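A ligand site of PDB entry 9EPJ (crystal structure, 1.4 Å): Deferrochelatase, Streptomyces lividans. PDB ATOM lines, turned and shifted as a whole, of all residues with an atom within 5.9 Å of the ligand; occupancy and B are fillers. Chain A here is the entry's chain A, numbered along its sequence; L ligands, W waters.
FE1 of the ligand is bound by NE2 of His 279 (2.1 Å). NE of Arg 195 is in salt-bridge range of O3 of the ligand (2.9 Å). The backbone NH of Gly 193 is in hydrogen-bond range of an oxygen (O1) of the ligand. An oxygen (O1) of the ligand is in hydrogen-bond range of the backbone NH (N) of Thr 194. The backbone NH (N) of Arg 195 sits at hydrogen-bond distance from an oxygen (O2) of the ligand (3.1 Å). The guanidinium group (NH1) of Arg 295 is in salt-bridge range of an oxygen (O1) of the ligand.
The backbone carbonyl oxygen (O) of Arg 229 is in hydrogen-bond range of the backbone NH (N) of Phe 316 (2.8 Å). ND2 of Asn 186 is in hydrogen-bond range of OD2 of Asp 192, at 2.9 Å. The backbone NH of Val 280 sits at hydrogen-bond distance from the backbone carbonyl oxygen of Phe 250, at 3.1 Å. OD1 of Asn 186 is in hydrogen-bond range of N of Leu 188 (2.9 Å). The guanidinium group (NH1) of Arg 195 is in hydrogen-bond range of a ring nitrogen (NE2) of His 284 (3.3 Å). The backbone NH (N) of Arg 295 lies within hydrogen-bond range of the side-chain amide oxygen (OD1) of Asn 196 (2.8 Å). The side-chain amide nitrogen (ND2) of Asn 186 sits close to the backbone carbonyl oxygen (O) of Phe 190 (3.5 Å). OD1 of Asp 192 is in salt-bridge range of NH1 of Arg 295, 3.2 Å away.
ND2 of Asn 186 touches C17 of the ligand, at 3.5 Å. CD1 of Leu 188 touches C17 of the ligand, at 3.8 Å. CB of Phe 190 touches C9 of the ligand, at 3.7 Å. O of Lys 191 touches C9 of the ligand (3.2 Å). OD2 of Asp 192 touches C2 of the ligand, 3.6 Å away. CG2 of Ile 231 touches C19 of the ligand (3.9 Å). Met 233 touches the ligand. CE1 of Phe 250 touches C2 of the ligand (3.4 Å). Arg 252 touches the ligand (CD to C10, 3.8 Å). Val 280 touches the ligand. Ala 283 touches the ligand. His 284 touches the ligand (CD2 to O3, 3.5 Å). Pro 285 touches the ligand (CD to O4, 3.1 Å). CB of Leu 314 touches C19 of the ligand, at 3.9 Å. CZ of Phe 316 touches C22 of the ligand, at 3.4 Å. Phe 327 touches the ligand (CE1 to C26, 3.4 Å). Val 330 touches the ligand (CG1 to C25, 3.9 Å). OE1 of Gln 331 touches C26 of the ligand, at 3.5 Å. Leu 334 touches the ligand (CD1 to C22, 3.9 Å). Leu 339 touches the ligand (CD2 to C15, 3.6 Å). CG2 of Ile 343 touches C19 of the ligand, at 3.97 Å. Hydrophobic or aromatic side chains that line the ligand: Leu 188, Phe 190, Ile 231, Met 233, Phe 250, His 279, Val 280, Ala 283, His 284, Pro 285, Leu 314, Phe 316, Phe 327, Val 330, Leu 334, Leu 339 and Ile 343. Within 4 Å of the ligand: Asn 186, Leu 188, Phe 190, Lys 191, Asp 192, Gly 193, Thr 194, Arg 195, Ile 231, Met 233, Phe 250, Arg 252, His 279, Val 280, Ala 283, His 284, Pro 285, Arg 295, Leu 314, Phe 316, Phe 327, Val 330, Gln 331, Leu 334, Leu 339 and Ile 343. The nearest printed residue that does not touch the ligand is Leu 293 (4.002 Å).
Water W1 lies within hydrogen-bond range of the side-chain carboxylate (OD1) of Asp 192 and the guanidinium group (NH1) of Arg 295. Water W3 lies within hydrogen-bond range of O3 of the ligand (2.7 Å) and NH2 of Arg 252 (2.8 Å). Water W5 bridges an oxygen (O4) of the ligand (2.7 Å) and the backbone carbonyl oxygen of Arg 195 (2.8 Å). Water W4 lies within hydrogen-bond range of a ring nitrogen (NE2) of His 345 and the side-chain amide oxygen of Gln 331.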
ATOM      1  N   ASN A 186     -13.405   4.608 -21.847  1.00  0.00           N
ATOM      2  CA  ASN A 186     -14.299   3.443 -21.850  1.00  0.00           C
ATOM      3  C   ASN A 186     -14.452   2.916 -20.404  1.00  0.00           C
ATOM      4  O   ASN A 186     -13.860   3.451 -19.473  1.00  0.00           O
ATOM      5  CB  ASN A 186     -13.800   2.381 -22.808  1.00  0.00           C
ATOM      6  CG  ASN A 186     -12.405   1.947 -22.492  1.00  0.00           C
ATOM      7  OD1 ASN A 186     -12.076   1.658 -21.321  1.00  0.00           O
ATOM      8  ND2 ASN A 186     -11.583   1.868 -23.538  1.00  0.00           N
ATOM      9  N   LEU A 188     -13.335   0.297 -19.037  1.00  0.00           N
ATOM     10  CA  LEU A 188     -12.121  -0.237 -18.433  1.00  0.00           C
ATOM     11  C   LEU A 188     -11.258   0.885 -17.871  1.00  0.00           C
ATOM     12  O   LEU A 188     -10.228   0.607 -17.263  1.00  0.00           O
ATOM     13  CB  LEU A 188     -11.330  -1.046 -19.441  1.00  0.00           C
ATOM     14  CG  LEU A 188     -12.058  -2.193 -20.126  1.00  0.00           C
ATOM     15  CD1 LEU A 188     -11.112  -2.971 -21.030  1.00  0.00           C
ATOM     16  CD2 LEU A 188     -12.723  -3.114 -19.103  1.00  0.00           C
ATOM     17  N   PHE A 190      -9.715   3.440 -19.521  1.00  0.00           N
ATOM     18  CA  PHE A 190      -8.711   3.988 -20.413  1.00  0.00           C
ATOM     19  C   PHE A 190      -9.333   4.930 -21.421  1.00  0.00           C
ATOM     20  O   PHE A 190     -10.415   4.698 -21.921  1.00  0.00           O
ATOM     21  CB  PHE A 190      -8.024   2.844 -21.152  1.00  0.00           C
ATOM     22  CG  PHE A 190      -6.948   2.165 -20.350  1.00  0.00           C
ATOM     23  CD1 PHE A 190      -7.254   1.318 -19.301  1.00  0.00           C
ATOM     24  CD2 PHE A 190      -5.601   2.436 -20.602  1.00  0.00           C
ATOM     25  CE1 PHE A 190      -6.243   0.697 -18.567  1.00  0.00           C
ATOM     26  CE2 PHE A 190      -4.622   1.859 -19.829  1.00  0.00           C
ATOM     27  CZ  PHE A 190      -4.921   1.012 -18.816  1.00  0.00           C
ATOM     28  N   LYS A 191      -8.579   5.962 -21.785  1.00  0.00           N
ATOM     29  CA  LYS A 191      -8.923   6.839 -22.862  1.00  0.00           C
ATOM     30  C   LYS A 191      -8.999   6.034 -24.160  1.00  0.00           C
ATOM     31  O   LYS A 191      -8.150   5.182 -24.407  1.00  0.00           O
ATOM     32  CB  LYS A 191      -7.867   7.931 -23.050  1.00  0.00           C
ATOM     33  CG  LYS A 191      -7.787   8.923 -21.919  1.00  0.00           C
ATOM     34  CD  LYS A 191      -6.642   9.928 -22.184  1.00  0.00           C
ATOM     35  CE  LYS A 191      -6.563  11.003 -21.140  1.00  0.00           C
ATOM     36  NZ  LYS A 191      -5.383  11.878 -21.324  1.00  0.00           N
ATOM     37  N   ASP A 192     -10.026   6.284 -24.958  1.00  0.00           N
ATOM     38  CA  ASP A 192     -10.303   5.519 -26.157  1.00  0.00           C
ATOM     39  C   ASP A 192     -10.658   6.498 -27.239  1.00  0.00           C
ATOM     40  O   ASP A 192     -11.643   7.207 -27.117  1.00  0.00           O
ATOM     41  CB  ASP A 192     -11.437   4.544 -25.875  1.00  0.00           C
ATOM     42  CG  ASP A 192     -11.499   3.318 -26.751  1.00  0.00           C
ATOM     43  OD1 ASP A 192     -10.930   3.317 -27.840  1.00  0.00           O
ATOM     44  OD2 ASP A 192     -12.158   2.384 -26.298  1.00  0.00           O
ATOM     45  N   GLY A 193      -9.769   6.621 -28.237  1.00  0.00           N
ATOM     46  CA  GLY A 193      -9.952   7.519 -29.359  1.00  0.00           C
ATOM     47  C   GLY A 193      -8.751   8.388 -29.642  1.00  0.00           C
ATOM     48  O   GLY A 193      -8.864   9.189 -30.544  1.00  0.00           O
ATOM     49  N   THR A 194      -7.647   8.279 -28.913  1.00  0.00           N
ATOM     50  CA  THR A 194      -6.506   9.141 -29.134  1.00  0.00           C
ATOM     51  C   THR A 194      -6.041   9.123 -30.595  1.00  0.00           C
ATOM     52  O   THR A 194      -5.863  10.182 -31.179  1.00  0.00           O
ATOM     53  CB  THR A 194      -5.390   8.737 -28.192  1.00  0.00           C
ATOM     54  OG1 THR A 194      -5.867   8.779 -26.858  1.00  0.00           O
ATOM     55  CG2 THR A 194      -4.153   9.599 -28.371  1.00  0.00           C
ATOM     56  N   ARG A 195      -5.742   7.945 -31.112  1.00  0.00           N
ATOM     57  CA  ARG A 195      -5.223   7.805 -32.456  1.00  0.00           C
ATOM     58  C   ARG A 195      -6.325   7.292 -33.373  1.00  0.00           C
ATOM     59  O   ARG A 195      -6.399   6.103 -33.687  1.00  0.00           O
ATOM     60  CB  ARG A 195      -3.963   6.934 -32.525  1.00  0.00           C
ATOM     61  CG  ARG A 195      -2.712   7.704 -32.178  1.00  0.00           C
ATOM     62  CD  ARG A 195      -1.422   6.943 -32.126  1.00  0.00           C
ATOM     63  NE  ARG A 195      -1.327   6.030 -33.264  1.00  0.00           N
ATOM     64  CZ  ARG A 195      -1.231   6.373 -34.529  1.00  0.00           C
ATOM     65  NH1 ARG A 195      -1.563   5.520 -35.447  1.00  0.00           N
ATOM     66  NH2 ARG A 195      -0.814   7.587 -34.871  1.00  0.00           N
ATOM     67  N   ASN A 196      -7.177   8.212 -33.802  1.00  0.00           N
ATOM     68  CA  ASN A 196      -8.282   7.917 -34.681  1.00  0.00           C
ATOM     69  C   ASN A 196      -8.039   8.688 -35.979  1.00  0.00           C
ATOM     70  O   ASN A 196      -6.896   8.742 -36.490  1.00  0.00           O
ATOM     71  CB  ASN A 196      -9.584   8.096 -33.890  1.00  0.00           C
ATOM     72  CG  ASN A 196     -10.767   7.451 -34.580  1.00  0.00           C
ATOM     73  OD1 ASN A 196     -10.696   6.369 -35.163  1.00  0.00           O
ATOM     74  ND2 ASN A 196     -11.900   8.101 -34.520  1.00  0.00           N
ATOM     75  N   ARG A 229     -19.795  -4.125 -33.782  1.00  0.00           N
ATOM     76  CA  ARG A 229     -19.575  -5.277 -32.915  1.00  0.00           C
ATOM     77  C   ARG A 229     -20.022  -4.967 -31.503  1.00  0.00           C
ATOM     78  O   ARG A 229     -19.583  -3.988 -30.903  1.00  0.00           O
ATOM     79  CB  ARG A 229     -18.101  -5.662 -32.914  1.00  0.00           C
ATOM     80  CG  ARG A 229     -17.513  -5.998 -34.261  1.00  0.00           C
ATOM     81  CD  ARG A 229     -17.969  -7.322 -34.858  1.00  0.00           C
ATOM     82  NE  ARG A 229     -17.262  -8.407 -34.172  1.00  0.00           N
ATOM     83  CZ  ARG A 229     -17.155  -9.644 -34.618  1.00  0.00           C
ATOM     84  NH1 ARG A 229     -17.781 -10.001 -35.731  1.00  0.00           N
ATOM     85  NH2 ARG A 229     -16.343 -10.481 -33.957  1.00  0.00           N
ATOM     86  N   ILE A 231     -19.611  -5.824 -27.844  1.00  0.00           N
ATOM     87  CA  ILE A 231     -18.531  -6.465 -27.122  1.00  0.00           C
ATOM     88  C   ILE A 231     -18.811  -6.409 -25.628  1.00  0.00           C
ATOM     89  O   ILE A 231     -18.918  -5.332 -25.039  1.00  0.00           O
ATOM     90  CB  ILE A 231     -17.172  -5.816 -27.451  1.00  0.00           C
ATOM     91  CG1 ILE A 231     -16.934  -5.748 -28.912  1.00  0.00           C
ATOM     92  CG2 ILE A 231     -16.025  -6.541 -26.729  1.00  0.00           C
ATOM     93  CD1 ILE A 231     -15.657  -5.011 -29.301  1.00  0.00           C
ATOM     94  N   MET A 233     -17.732  -6.838 -21.766  1.00  0.00           N
ATOM     95  CA  MET A 233     -16.502  -6.685 -21.006  1.00  0.00           C
ATOM     96  C   MET A 233     -16.630  -7.499 -19.731  1.00  0.00           C
ATOM     97  O   MET A 233     -17.623  -7.429 -19.047  1.00  0.00           O
ATOM     98  CB  MET A 233     -16.267  -5.222 -20.633  1.00  0.00           C
ATOM     99  CG  MET A 233     -15.883  -4.375 -21.798  1.00  0.00           C
ATOM    100  SD  MET A 233     -15.944  -2.620 -21.310  1.00  0.00           S
ATOM    101  CE  MET A 233     -14.954  -1.858 -22.605  1.00  0.00           C
ATOM    102  N   PHE A 250      -2.761  -2.732 -22.776  1.00  0.00           N
ATOM    103  CA  PHE A 250      -2.951  -1.711 -23.793  1.00  0.00           C
ATOM    104  C   PHE A 250      -1.657  -1.204 -24.427  1.00  0.00           C
ATOM    105  O   PHE A 250      -1.639  -0.949 -25.634  1.00  0.00           O
ATOM    106  CB  PHE A 250      -3.788  -0.552 -23.248  1.00  0.00           C
ATOM    107  CG  PHE A 250      -5.244  -0.938 -23.145  1.00  0.00           C
ATOM    108  CD1 PHE A 250      -5.955  -1.179 -24.304  1.00  0.00           C
ATOM    109  CD2 PHE A 250      -5.873  -1.074 -21.929  1.00  0.00           C
ATOM    110  CE1 PHE A 250      -7.249  -1.611 -24.248  1.00  0.00           C
ATOM    111  CE2 PHE A 250      -7.203  -1.501 -21.877  1.00  0.00           C
ATOM    112  CZ  PHE A 250      -7.865  -1.764 -23.038  1.00  0.00           C
ATOM    113  N   ARG A 252      -0.411   1.655 -23.059  1.00  0.00           N
ATOM    114  CA  ARG A 252      -0.501   3.045 -22.641  1.00  0.00           C
ATOM    115  C   ARG A 252      -0.756   3.056 -21.148  1.00  0.00           C
ATOM    116  O   ARG A 252      -1.281   2.078 -20.628  1.00  0.00           O
ATOM    117  CB  ARG A 252      -1.647   3.751 -23.341  1.00  0.00           C
ATOM    118  CG  ARG A 252      -1.372   4.026 -24.795  1.00  0.00           C
ATOM    119  CD  ARG A 252      -2.538   4.674 -25.498  1.00  0.00           C
ATOM    120  NE  ARG A 252      -2.254   5.081 -26.876  1.00  0.00           N
ATOM    121  CZ  ARG A 252      -1.753   6.222 -27.293  1.00  0.00           C
ATOM    122  NH1 ARG A 252      -1.388   7.189 -26.456  1.00  0.00           N
ATOM    123  NH2 ARG A 252      -1.684   6.426 -28.592  1.00  0.00           N
ATOM    124  N   PRO A 269       3.272   6.542 -30.301  1.00  0.00           N
ATOM    125  CA  PRO A 269       3.713   5.276 -29.765  1.00  0.00           C
ATOM    126  C   PRO A 269       5.056   4.829 -30.313  1.00  0.00           C
ATOM    127  O   PRO A 269       5.301   5.016 -31.486  1.00  0.00           O
ATOM    128  CB  PRO A 269       2.632   4.282 -30.153  1.00  0.00           C
ATOM    129  CG  PRO A 269       1.575   5.069 -30.807  1.00  0.00           C
ATOM    130  CD  PRO A 269       2.004   6.504 -31.008  1.00  0.00           C
ATOM    131  N   HIS A 279      -2.612  -4.376 -26.997  1.00  0.00           N
ATOM    132  CA  HIS A 279      -3.654  -3.980 -27.931  1.00  0.00           C
ATOM    133  C   HIS A 279      -3.194  -2.934 -28.930  1.00  0.00           C
ATOM    134  O   HIS A 279      -3.491  -3.070 -30.111  1.00  0.00           O
ATOM    135  CB  HIS A 279      -4.891  -3.563 -27.134  1.00  0.00           C
ATOM    136  CG  HIS A 279      -6.048  -3.163 -27.956  1.00  0.00           C
ATOM    137  ND1 HIS A 279      -6.853  -4.052 -28.622  1.00  0.00           N
ATOM    138  CD2 HIS A 279      -6.553  -1.917 -28.227  1.00  0.00           C
ATOM    139  CE1 HIS A 279      -7.782  -3.356 -29.295  1.00  0.00           C
ATOM    140  NE2 HIS A 279      -7.655  -2.057 -29.039  1.00  0.00           N
ATOM    141  N   VAL A 280      -2.586  -1.852 -28.443  1.00  0.00           N
ATOM    142  CA  VAL A 280      -2.172  -0.774 -29.320  1.00  0.00           C
ATOM    143  C   VAL A 280      -1.153  -1.280 -30.312  1.00  0.00           C
ATOM    144  O   VAL A 280      -1.213  -0.880 -31.456  1.00  0.00           O
ATOM    145  CB  VAL A 280      -1.683   0.439 -28.540  1.00  0.00           C
ATOM    146  CG1 VAL A 280      -1.028   1.477 -29.434  1.00  0.00           C
ATOM    147  CG2 VAL A 280      -2.830   1.068 -27.762  1.00  0.00           C
ATOM    148  N   ALA A 283      -3.022  -3.352 -32.978  1.00  0.00           N
ATOM    149  CA  ALA A 283      -4.036  -2.624 -33.732  1.00  0.00           C
ATOM    150  C   ALA A 283      -3.470  -1.503 -34.570  1.00  0.00           C
ATOM    151  O   ALA A 283      -4.189  -1.000 -35.437  1.00  0.00           O
ATOM    152  CB  ALA A 283      -5.086  -2.055 -32.769  1.00  0.00           C
ATOM    153  N   HIS A 284      -2.248  -1.054 -34.291  1.00  0.00           N
ATOM    154  CA  HIS A 284      -1.673   0.133 -34.933  1.00  0.00           C
ATOM    155  C   HIS A 284      -1.545  -0.091 -36.433  1.00  0.00           C
ATOM    156  O   HIS A 284      -1.244  -1.195 -36.850  1.00  0.00           O
ATOM    157  CB  HIS A 284      -0.290   0.377 -34.335  1.00  0.00           C
ATOM    158  CG  HIS A 284       0.281   1.700 -34.628  1.00  0.00           C
ATOM    159  ND1 HIS A 284       0.916   1.979 -35.834  1.00  0.00           N
ATOM    160  CD2 HIS A 284       0.420   2.804 -33.868  1.00  0.00           C
ATOM    161  CE1 HIS A 284       1.364   3.217 -35.812  1.00  0.00           C
ATOM    162  NE2 HIS A 284       1.085   3.754 -34.624  1.00  0.00           N
ATOM    163  N   PRO A 285      -1.795   0.935 -37.276  1.00  0.00           N
ATOM    164  CA  PRO A 285      -1.647   0.813 -38.718  1.00  0.00           C
ATOM    165  C   PRO A 285      -0.309   0.215 -39.143  1.00  0.00           C
ATOM    166  O   PRO A 285      -0.301  -0.570 -40.092  1.00  0.00           O
ATOM    167  CB  PRO A 285      -1.827   2.256 -39.189  1.00  0.00           C
ATOM    168  CG  PRO A 285      -2.794   2.817 -38.199  1.00  0.00           C
ATOM    169  CD  PRO A 285      -2.302   2.273 -36.900  1.00  0.00           C
ATOM    170  N   LEU A 293      -8.650   2.808 -39.399  1.00  0.00           N
ATOM    171  CA  LEU A 293     -10.099   2.792 -39.250  1.00  0.00           C
ATOM    172  C   LEU A 293     -10.545   4.104 -38.648  1.00  0.00           C
ATOM    173  O   LEU A 293      -9.795   4.750 -37.937  1.00  0.00           O
ATOM    174  CB  LEU A 293     -10.479   1.733 -38.201  1.00  0.00           C
ATOM    175  CG  LEU A 293     -10.044   0.301 -38.421  1.00  0.00           C
ATOM    176  CD1 LEU A 293     -10.427  -0.564 -37.234  1.00  0.00           C
ATOM    177  CD2 LEU A 293     -10.748  -0.203 -39.664  1.00  0.00           C
ATOM    178  N   ARG A 295     -12.956   4.880 -35.796  1.00  0.00           N
ATOM    179  CA  ARG A 295     -13.674   4.271 -34.710  1.00  0.00           C
ATOM    180  C   ARG A 295     -14.646   5.261 -34.135  1.00  0.00           C
ATOM    181  O   ARG A 295     -14.298   6.431 -33.943  1.00  0.00           O
ATOM    182  CB  ARG A 295     -12.712   3.843 -33.605  1.00  0.00           C
ATOM    183  CG  ARG A 295     -11.811   2.710 -34.047  1.00  0.00           C
ATOM    184  CD  ARG A 295     -10.823   2.324 -33.010  1.00  0.00           C
ATOM    185  NE  ARG A 295      -9.790   3.352 -32.953  1.00  0.00           N
ATOM    186  CZ  ARG A 295      -9.234   3.852 -31.882  1.00  0.00           C
ATOM    187  NH1 ARG A 295      -9.602   3.466 -30.697  1.00  0.00           N
ATOM    188  NH2 ARG A 295      -8.311   4.797 -31.985  1.00  0.00           N
ATOM    189  N   LEU A 314     -19.054  -2.496 -24.723  1.00  0.00           N
ATOM    190  CA  LEU A 314     -18.682  -1.484 -25.690  1.00  0.00           C
ATOM    191  C   LEU A 314     -19.322  -1.864 -27.008  1.00  0.00           C
ATOM    192  O   LEU A 314     -19.178  -2.979 -27.483  1.00  0.00           O
ATOM    193  CB  LEU A 314     -17.159  -1.362 -25.752  1.00  0.00           C
ATOM    194  CG  LEU A 314     -16.610  -0.099 -26.402  1.00  0.00           C
ATOM    195  CD1 LEU A 314     -15.283   0.274 -25.830  1.00  0.00           C
ATOM    196  CD2 LEU A 314     -16.512  -0.252 -27.886  1.00  0.00           C
ATOM    197  N   PHE A 316     -18.925  -1.310 -30.508  1.00  0.00           N
ATOM    198  CA  PHE A 316     -17.807  -0.874 -31.324  1.00  0.00           C
ATOM    199  C   PHE A 316     -18.318  -0.584 -32.717  1.00  0.00           C
ATOM    200  O   PHE A 316     -18.979  -1.419 -33.297  1.00  0.00           O
ATOM    201  CB  PHE A 316     -16.778  -2.014 -31.351  1.00  0.00           C
ATOM    202  CG  PHE A 316     -15.565  -1.653 -32.170  1.00  0.00           C
ATOM    203  CD1 PHE A 316     -14.529  -0.941 -31.574  1.00  0.00           C
ATOM    204  CD2 PHE A 316     -15.449  -2.015 -33.498  1.00  0.00           C
ATOM    205  CE1 PHE A 316     -13.373  -0.636 -32.299  1.00  0.00           C
ATOM    206  CE2 PHE A 316     -14.318  -1.675 -34.211  1.00  0.00           C
ATOM    207  CZ  PHE A 316     -13.297  -0.995 -33.586  1.00  0.00           C
ATOM    208  N   PHE A 327     -11.414  -3.242 -41.139  1.00  0.00           N
ATOM    209  CA  PHE A 327     -11.688  -4.021 -39.948  1.00  0.00           C
ATOM    210  C   PHE A 327     -11.101  -5.436 -40.031  1.00  0.00           C
ATOM    211  O   PHE A 327     -10.579  -5.931 -39.046  1.00  0.00           O
ATOM    212  CB  PHE A 327     -13.192  -4.088 -39.730  1.00  0.00           C
ATOM    213  CG  PHE A 327     -13.616  -4.909 -38.522  1.00  0.00           C
ATOM    214  CD1 PHE A 327     -13.545  -4.341 -37.259  1.00  0.00           C
ATOM    215  CD2 PHE A 327     -13.913  -6.259 -38.619  1.00  0.00           C
ATOM    216  CE1 PHE A 327     -13.851  -5.074 -36.130  1.00  0.00           C
ATOM    217  CE2 PHE A 327     -14.256  -6.975 -37.483  1.00  0.00           C
ATOM    218  CZ  PHE A 327     -14.202  -6.402 -36.233  1.00  0.00           C
ATOM    219  N   VAL A 330      -7.289  -5.830 -39.200  1.00  0.00           N
ATOM    220  CA  VAL A 330      -6.960  -5.415 -37.875  1.00  0.00           C
ATOM    221  C   VAL A 330      -7.531  -6.427 -36.888  1.00  0.00           C
ATOM    222  O   VAL A 330      -6.812  -6.868 -35.987  1.00  0.00           O
ATOM    223  CB  VAL A 330      -7.432  -3.984 -37.626  1.00  0.00           C
ATOM    224  CG1 VAL A 330      -7.177  -3.573 -36.198  1.00  0.00           C
ATOM    225  CG2 VAL A 330      -6.773  -3.029 -38.600  1.00  0.00           C
ATOM    226  N   GLN A 331      -8.795  -6.844 -37.035  1.00  0.00           N
ATOM    227  CA  GLN A 331      -9.335  -7.814 -36.107  1.00  0.00           C
ATOM    228  C   GLN A 331      -8.583  -9.158 -36.202  1.00  0.00           C
ATOM    229  O   GLN A 331      -8.391  -9.817 -35.192  1.00  0.00           O
ATOM    230  CB  GLN A 331     -10.863  -7.965 -36.322  1.00  0.00           C
ATOM    231  CG  GLN A 331     -11.576  -8.955 -35.421  1.00  0.00           C
ATOM    232  CD  GLN A 331     -11.494  -8.637 -33.944  1.00  0.00           C
ATOM    233  OE1 GLN A 331     -11.490  -7.479 -33.541  1.00  0.00           O
ATOM    234  NE2 GLN A 331     -11.453  -9.666 -33.122  1.00  0.00           N
ATOM    235  N   LEU A 334      -5.728  -9.103 -34.020  1.00  0.00           N
ATOM    236  CA  LEU A 334      -6.030  -9.095 -32.594  1.00  0.00           C
ATOM    237  C   LEU A 334      -6.269 -10.502 -32.063  1.00  0.00           C
ATOM    238  O   LEU A 334      -6.670 -10.669 -30.903  1.00  0.00           O
ATOM    239  CB  LEU A 334      -7.225  -8.202 -32.268  1.00  0.00           C
ATOM    240  CG  LEU A 334      -7.039  -6.731 -32.649  1.00  0.00           C
ATOM    241  CD1 LEU A 334      -8.264  -5.905 -32.164  1.00  0.00           C
ATOM    242  CD2 LEU A 334      -5.816  -6.122 -32.113  1.00  0.00           C
ATOM    243  N   LEU A 339      -6.008  -8.184 -24.607  1.00  0.00           N
ATOM    244  CA  LEU A 339      -7.334  -7.718 -24.267  1.00  0.00           C
ATOM    245  C   LEU A 339      -8.375  -8.821 -24.387  1.00  0.00           C
ATOM    246  O   LEU A 339      -9.417  -8.778 -23.724  1.00  0.00           O
ATOM    247  CB  LEU A 339      -7.714  -6.547 -25.156  1.00  0.00           C
ATOM    248  CG  LEU A 339      -9.032  -5.853 -24.817  1.00  0.00           C
ATOM    249  CD1 LEU A 339      -9.099  -5.308 -23.409  1.00  0.00           C
ATOM    250  CD2 LEU A 339      -9.301  -4.765 -25.839  1.00  0.00           C
ATOM    251  N   ILE A 343     -12.756  -9.608 -22.823  1.00  0.00           N
ATOM    252  CA  ILE A 343     -13.857  -9.206 -23.683  1.00  0.00           C
ATOM    253  C   ILE A 343     -14.397 -10.421 -24.416  1.00  0.00           C
ATOM    254  O   ILE A 343     -13.736 -11.436 -24.495  1.00  0.00           O
ATOM    255  CB  ILE A 343     -13.439  -8.134 -24.695  1.00  0.00           C
ATOM    256  CG1 ILE A 343     -12.419  -8.662 -25.688  1.00  0.00           C
ATOM    257  CG2 ILE A 343     -12.965  -6.884 -23.985  1.00  0.00           C
ATOM    258  CD1 ILE A 343     -12.237  -7.760 -26.898  1.00  0.00           C
ATOM    259  N   HIS A 345     -16.866 -10.816 -28.125  1.00  0.00           N
ATOM    260  CA  HIS A 345     -17.769 -10.282 -29.124  1.00  0.00           C
ATOM    261  C   HIS A 345     -19.037 -11.122 -29.130  1.00  0.00           C
ATOM    262  O   HIS A 345     -18.952 -12.338 -29.344  1.00  0.00           O
ATOM    263  CB  HIS A 345     -17.102 -10.276 -30.472  1.00  0.00           C
ATOM    264  CG  HIS A 345     -15.916  -9.389 -30.580  1.00  0.00           C
ATOM    265  ND1 HIS A 345     -15.835  -8.488 -31.619  1.00  0.00           N
ATOM    266  CD2 HIS A 345     -14.789  -9.295 -29.893  1.00  0.00           C
ATOM    267  CE1 HIS A 345     -14.679  -7.834 -31.517  1.00  0.00           C
ATOM    268  NE2 HIS A 345     -14.000  -8.346 -30.497  1.00  0.00           N
HETATM  269  C1  LIG L   1      -6.716   1.842 -29.643  1.00  0.00           C
HETATM  270  C2  LIG L   1      -9.492   0.025 -26.159  1.00  0.00           C
HETATM  271  C3  LIG L   1     -11.611  -2.921 -29.328  1.00  0.00           C
HETATM  272  C4  LIG L   1      -8.914  -0.980 -32.805  1.00  0.00           C
HETATM  273  C5  LIG L   1      -7.239   1.600 -28.401  1.00  0.00           C
HETATM  274  C6  LIG L   1      -6.866   2.269 -27.206  1.00  0.00           C
HETATM  275  C7  LIG L   1      -7.642   1.746 -26.202  1.00  0.00           C
HETATM  276  C8  LIG L   1      -8.493   0.787 -26.813  1.00  0.00           C
HETATM  277  C9  LIG L   1      -7.613   2.076 -24.721  1.00  0.00           C
HETATM  278  C10 LIG L   1      -5.769   3.296 -27.069  1.00  0.00           C
HETATM  279  C11 LIG L   1      -6.180   4.745 -27.339  1.00  0.00           C
HETATM  280  C12 LIG L   1      -6.568   5.006 -28.726  1.00  0.00           C
HETATM  281  O1  LIG L   1      -7.776   4.966 -29.084  1.00  0.00           O
HETATM  282  O2  LIG L   1      -5.711   5.299 -29.595  1.00  0.00           O
HETATM  283  C13 LIG L   1     -10.339  -0.907 -26.738  1.00  0.00           C
HETATM  284  C14 LIG L   1     -11.323  -1.644 -25.981  1.00  0.00           C
HETATM  285  C15 LIG L   1     -11.904  -2.475 -26.877  1.00  0.00           C
HETATM  286  C16 LIG L   1     -11.267  -2.270 -28.174  1.00  0.00           C
HETATM  287  C17 LIG L   1     -11.605  -1.511 -24.496  1.00  0.00           C
HETATM  288  C18 LIG L   1     -13.022  -3.442 -26.747  1.00  0.00           C
HETATM  289  C19 LIG L   1     -13.873  -3.465 -25.777  1.00  0.00           C
HETATM  290  C20 LIG L   1     -11.062  -2.701 -30.571  1.00  0.00           C
HETATM  291  C21 LIG L   1     -11.370  -3.377 -31.776  1.00  0.00           C
HETATM  292  C22 LIG L   1     -10.615  -2.832 -32.770  1.00  0.00           C
HETATM  293  C23 LIG L   1      -9.777  -1.824 -32.163  1.00  0.00           C
HETATM  294  C24 LIG L   1     -12.408  -4.409 -31.863  1.00  0.00           C
HETATM  295  C25 LIG L   1     -10.507  -3.165 -34.194  1.00  0.00           C
HETATM  296  C26 LIG L   1     -10.852  -4.251 -34.742  1.00  0.00           C
HETATM  297  C27 LIG L   1      -8.141   0.009 -32.211  1.00  0.00           C
HETATM  298  C28 LIG L   1      -7.217   0.856 -32.982  1.00  0.00           C
HETATM  299  C29 LIG L   1      -6.549   1.623 -32.118  1.00  0.00           C
HETATM  300  C30 LIG L   1      -7.113   1.248 -30.792  1.00  0.00           C
HETATM  301  C31 LIG L   1      -7.069   0.830 -34.501  1.00  0.00           C
HETATM  302  C32 LIG L   1      -5.551   2.684 -32.366  1.00  0.00           C
HETATM  303  C33 LIG L   1      -4.122   2.098 -32.469  1.00  0.00           C
HETATM  304  C34 LIG L   1      -3.150   3.132 -32.917  1.00  0.00           C
HETATM  305  O3  LIG L   1      -2.409   3.658 -32.047  1.00  0.00           O
HETATM  306  O4  LIG L   1      -3.158   3.476 -34.120  1.00  0.00           O
HETATM  307  N1  LIG L   1      -8.260   0.695 -28.140  1.00  0.00           N
HETATM  308  N2  LIG L   1     -10.352  -1.300 -27.994  1.00  0.00           N
HETATM  309  N3  LIG L   1     -10.103  -1.747 -30.835  1.00  0.00           N
HETATM  310  N4  LIG L   1      -8.043   0.286 -30.909  1.00  0.00           N
HETATM  311 FE1  LIG L   1      -9.080  -0.579 -29.449  1.00  0.00          FE
HETATM  312  O   HOH W   1     -10.734   1.085 -29.522  1.00  0.00           O
HETATM  313  O   HOH W   2      -6.733   2.890 -37.149  1.00  0.00           O
HETATM  314  O   HOH W   3      -3.218   4.224 -29.544  1.00  0.00           O
HETATM  315  O   HOH W   4     -11.365  -7.450 -30.499  1.00  0.00           O
HETATM  316  O   HOH W   5      -5.128   4.616 -35.649  1.00  0.00           O
HETATM  317  O   HOH W   6      -5.569   0.345 -37.461  1.00  0.00           O
HETATM  318  O   HOH W   7     -13.038   0.666 -28.207  1.00  0.00           O
